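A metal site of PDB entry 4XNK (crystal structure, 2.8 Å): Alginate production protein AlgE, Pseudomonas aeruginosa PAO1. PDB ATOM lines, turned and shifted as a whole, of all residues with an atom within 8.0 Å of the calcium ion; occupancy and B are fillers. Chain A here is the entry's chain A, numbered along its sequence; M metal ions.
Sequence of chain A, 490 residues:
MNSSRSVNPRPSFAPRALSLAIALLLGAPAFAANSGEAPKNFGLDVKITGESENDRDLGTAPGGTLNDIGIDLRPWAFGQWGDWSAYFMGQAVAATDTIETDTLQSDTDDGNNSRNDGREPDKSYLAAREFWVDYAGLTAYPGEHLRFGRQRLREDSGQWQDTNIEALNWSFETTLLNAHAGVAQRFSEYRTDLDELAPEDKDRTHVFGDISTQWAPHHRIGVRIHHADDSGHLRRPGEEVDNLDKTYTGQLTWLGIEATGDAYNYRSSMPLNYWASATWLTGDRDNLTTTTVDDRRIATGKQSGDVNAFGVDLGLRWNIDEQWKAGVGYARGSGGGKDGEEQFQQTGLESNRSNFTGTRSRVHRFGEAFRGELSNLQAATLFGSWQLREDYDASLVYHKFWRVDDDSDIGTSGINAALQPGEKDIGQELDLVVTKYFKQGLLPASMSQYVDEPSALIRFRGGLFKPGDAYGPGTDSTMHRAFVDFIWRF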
ATOM      1  N   ASN A  54     -18.519 -17.587   2.635  1.00  0.00           N
ATOM      2  CA  ASN A  54     -17.708 -18.514   1.852  1.00  0.00           C
ATOM      3  C   ASN A  54     -17.907 -18.200   0.379  1.00  0.00           C
ATOM      4  O   ASN A  54     -18.387 -17.083   0.093  1.00  0.00           O
ATOM      5  CB  ASN A  54     -17.870 -19.990   2.196  1.00  0.00           C
ATOM      6  CG  ASN A  54     -16.483 -20.605   2.128  1.00  0.00           C
ATOM      7  OD1 ASN A  54     -16.054 -21.143   1.111  1.00  0.00           O
ATOM      8  ND2 ASN A  54     -15.716 -20.481   3.198  1.00  0.00           N
ATOM      9  N   ASP A  55     -17.479 -19.070  -0.555  1.00  0.00           N
ATOM     10  CA  ASP A  55     -17.500 -18.635  -1.939  1.00  0.00           C
ATOM     11  C   ASP A  55     -18.879 -18.307  -2.448  1.00  0.00           C
ATOM     12  O   ASP A  55     -19.673 -19.198  -2.724  1.00  0.00           O
ATOM     13  CB  ASP A  55     -16.742 -19.591  -2.855  1.00  0.00           C
ATOM     14  CG  ASP A  55     -15.745 -18.844  -3.700  1.00  0.00           C
ATOM     15  OD1 ASP A  55     -15.965 -17.643  -3.955  1.00  0.00           O
ATOM     16  OD2 ASP A  55     -14.778 -19.471  -4.180  1.00  0.00           O
ATOM     17  N   ARG A  56     -19.123 -16.977  -2.638  1.00  0.00           N
ATOM     18  CA  ARG A  56     -20.360 -16.432  -3.199  1.00  0.00           C
ATOM     19  C   ARG A  56     -20.505 -16.778  -4.700  1.00  0.00           C
ATOM     20  O   ARG A  56     -21.620 -16.772  -5.193  1.00  0.00           O
ATOM     21  CB  ARG A  56     -20.532 -14.933  -2.890  1.00  0.00           C
ATOM     22  CG  ARG A  56     -19.990 -13.949  -3.928  1.00  0.00           C
ATOM     23  CD  ARG A  56     -20.147 -12.522  -3.452  1.00  0.00           C
ATOM     24  NE  ARG A  56     -21.507 -12.023  -3.632  1.00  0.00           N
ATOM     25  CZ  ARG A  56     -21.916 -10.827  -3.233  1.00  0.00           C
ATOM     26  NH1 ARG A  56     -21.099 -10.008  -2.589  1.00  0.00           N
ATOM     27  NH2 ARG A  56     -23.170 -10.444  -3.463  1.00  0.00           N
ATOM     28  N   ASP A  57     -19.400 -17.089  -5.388  1.00  0.00           N
ATOM     29  CA  ASP A  57     -19.388 -17.497  -6.801  1.00  0.00           C
ATOM     30  C   ASP A  57     -19.376 -19.033  -6.942  1.00  0.00           C
ATOM     31  O   ASP A  57     -19.289 -19.563  -8.061  1.00  0.00           O
ATOM     32  CB  ASP A  57     -18.186 -16.872  -7.540  1.00  0.00           C
ATOM     33  CG  ASP A  57     -16.853 -17.051  -6.834  1.00  0.00           C
ATOM     34  OD1 ASP A  57     -16.301 -16.034  -6.355  1.00  0.00           O
ATOM     35  OD2 ASP A  57     -16.353 -18.182  -6.787  1.00  0.00           O
ATOM     36  N   LEU A  58     -19.475 -19.743  -5.781  1.00  0.00           N
ATOM     37  CA  LEU A  58     -19.495 -21.202  -5.636  1.00  0.00           C
ATOM     38  C   LEU A  58     -18.187 -21.879  -6.143  1.00  0.00           C
ATOM     39  O   LEU A  58     -18.220 -22.977  -6.699  1.00  0.00           O
ATOM     40  CB  LEU A  58     -20.771 -21.826  -6.265  1.00  0.00           C
ATOM     41  CG  LEU A  58     -22.145 -21.352  -5.733  1.00  0.00           C
ATOM     42  CD1 LEU A  58     -23.243 -21.714  -6.715  1.00  0.00           C
ATOM     43  CD2 LEU A  58     -22.468 -21.982  -4.391  1.00  0.00           C
ATOM     44  N   GLY A  59     -17.049 -21.239  -5.882  1.00  0.00           N
ATOM     45  CA  GLY A  59     -15.731 -21.736  -6.252  1.00  0.00           C
ATOM     46  C   GLY A  59     -15.447 -21.744  -7.740  1.00  0.00           C
ATOM     47  O   GLY A  59     -14.736 -22.634  -8.223  1.00  0.00           O
ATOM     48  N   THR A  60     -16.005 -20.760  -8.491  1.00  0.00           N
ATOM     49  CA  THR A  60     -15.843 -20.652  -9.944  1.00  0.00           C
ATOM     50  C   THR A  60     -15.126 -19.371 -10.427  1.00  0.00           C
ATOM     51  O   THR A  60     -14.916 -19.222 -11.638  1.00  0.00           O
ATOM     52  CB  THR A  60     -17.206 -20.817 -10.676  1.00  0.00           C
ATOM     53  OG1 THR A  60     -17.988 -19.623 -10.566  1.00  0.00           O
ATOM     54  CG2 THR A  60     -17.994 -22.049 -10.198  1.00  0.00           C
ATOM     55  N   ALA A  61     -14.764 -18.448  -9.509  1.00  0.00           N
ATOM     56  CA  ALA A  61     -14.120 -17.163  -9.840  1.00  0.00           C
ATOM     57  C   ALA A  61     -13.300 -16.586  -8.676  1.00  0.00           C
ATOM     58  O   ALA A  61     -13.700 -16.763  -7.532  1.00  0.00           O
ATOM     59  CB  ALA A  61     -15.182 -16.149 -10.249  1.00  0.00           C
ATOM     60  N   PRO A  62     -12.174 -15.846  -8.929  1.00  0.00           N
ATOM     61  CA  PRO A  62     -11.413 -15.260  -7.799  1.00  0.00           C
ATOM     62  C   PRO A  62     -12.259 -14.289  -6.979  1.00  0.00           C
ATOM     63  O   PRO A  62     -13.083 -13.568  -7.532  1.00  0.00           O
ATOM     64  CB  PRO A  62     -10.228 -14.558  -8.475  1.00  0.00           C
ATOM     65  CG  PRO A  62     -10.592 -14.419  -9.902  1.00  0.00           C
ATOM     66  CD  PRO A  62     -11.546 -15.521 -10.232  1.00  0.00           C
ATOM     67  N   GLY A  63     -12.065 -14.317  -5.668  1.00  0.00           N
ATOM     68  CA  GLY A  63     -12.821 -13.502  -4.724  1.00  0.00           C
ATOM     69  C   GLY A  63     -14.071 -14.197  -4.189  1.00  0.00           C
ATOM     70  O   GLY A  63     -14.172 -15.420  -4.257  1.00  0.00           O
ATOM     71  N   GLY A  64     -15.005 -13.416  -3.664  1.00  0.00           N
ATOM     72  CA  GLY A  64     -16.245 -13.926  -3.100  1.00  0.00           C
ATOM     73  C   GLY A  64     -16.077 -14.546  -1.734  1.00  0.00           C
ATOM     74  O   GLY A  64     -16.946 -15.298  -1.285  1.00  0.00           O
ATOM     75  N   THR A  65     -14.965 -14.236  -1.046  1.00  0.00           N
ATOM     76  CA  THR A  65     -14.661 -14.702   0.300  1.00  0.00           C
ATOM     77  C   THR A  65     -14.442 -13.467   1.191  1.00  0.00           C
ATOM     78  O   THR A  65     -13.719 -12.547   0.793  1.00  0.00           O
ATOM     79  CB  THR A  65     -13.442 -15.652   0.295  1.00  0.00           C
ATOM     80  OG1 THR A  65     -13.692 -16.746  -0.580  1.00  0.00           O
ATOM     81  CG2 THR A  65     -13.091 -16.181   1.673  1.00  0.00           C
ATOM     82  N   ASN A 416     -23.065 -15.426  -7.400  1.00  0.00           N
ATOM     83  CA  ASN A 416     -22.548 -14.939  -8.689  1.00  0.00           C
ATOM     84  C   ASN A 416     -21.883 -16.103  -9.430  1.00  0.00           C
ATOM     85  O   ASN A 416     -20.666 -16.144  -9.575  1.00  0.00           O
ATOM     86  CB  ASN A 416     -21.562 -13.765  -8.491  1.00  0.00           C
ATOM     87  CG  ASN A 416     -22.149 -12.492  -7.940  1.00  0.00           C
ATOM     88  OD1 ASN A 416     -22.894 -11.781  -8.625  1.00  0.00           O
ATOM     89  ND2 ASN A 416     -21.754 -12.127  -6.741  1.00  0.00           N
ATOM     90  N   ASP A 476     -18.844 -25.795  -5.270  1.00  0.00           N
ATOM     91  CA  ASP A 476     -18.672 -26.344  -3.914  1.00  0.00           C
ATOM     92  C   ASP A 476     -19.981 -26.929  -3.425  1.00  0.00           C
ATOM     93  O   ASP A 476     -21.043 -26.466  -3.852  1.00  0.00           O
ATOM     94  CB  ASP A 476     -18.190 -25.255  -2.942  1.00  0.00           C
ATOM     95  CG  ASP A 476     -16.915 -24.558  -3.355  1.00  0.00           C
ATOM     96  OD1 ASP A 476     -16.137 -25.157  -4.128  1.00  0.00           O
ATOM     97  OD2 ASP A 476     -16.694 -23.416  -2.908  1.00  0.00           O
HETATM   98 CA    CA M   1     -14.171 -17.477  -5.527  1.00  0.00          CA
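The side-chain carboxylate (OD2) of Asp 55 sits close to the backbone NH (N) of Gly 59 (3.3 Å).
N of Gly 59 lies close to OD2 of Asp 57 (3.3 Å).
The side-chain hydroxyl of Thr 60 lies within hydrogen-bond range of the backbone carbonyl oxygen of Asp 57, at 2.8 Å.
Merely in contact with the calcium ion: Pro 62 (3.99 Å).
Five residues have an atom within 4 Å of the calcium ion: Asp 55, Asp 57, Ala 61, Pro 62 and Gly 63.
The nearest printed residue that does not touch the calcium ion is Gly 64 (4.5 Å).
O of Ala 61 is bound to the calcium ion (2.2 Å).
OD1 of Asp 55 is bound to the calcium ion, at 2.4 Å.
O of Gly 63 is bound to the calcium ion (2.4 Å).
The side-chain carboxylate (OD2) of Asp 55 binds the calcium ion (2.5 Å).
The calcium ion is bound by OD2 of Asp 57 (2.6 Å).
The calcium ion is bound by OD1 of Asp 57, at 2.7 Å.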
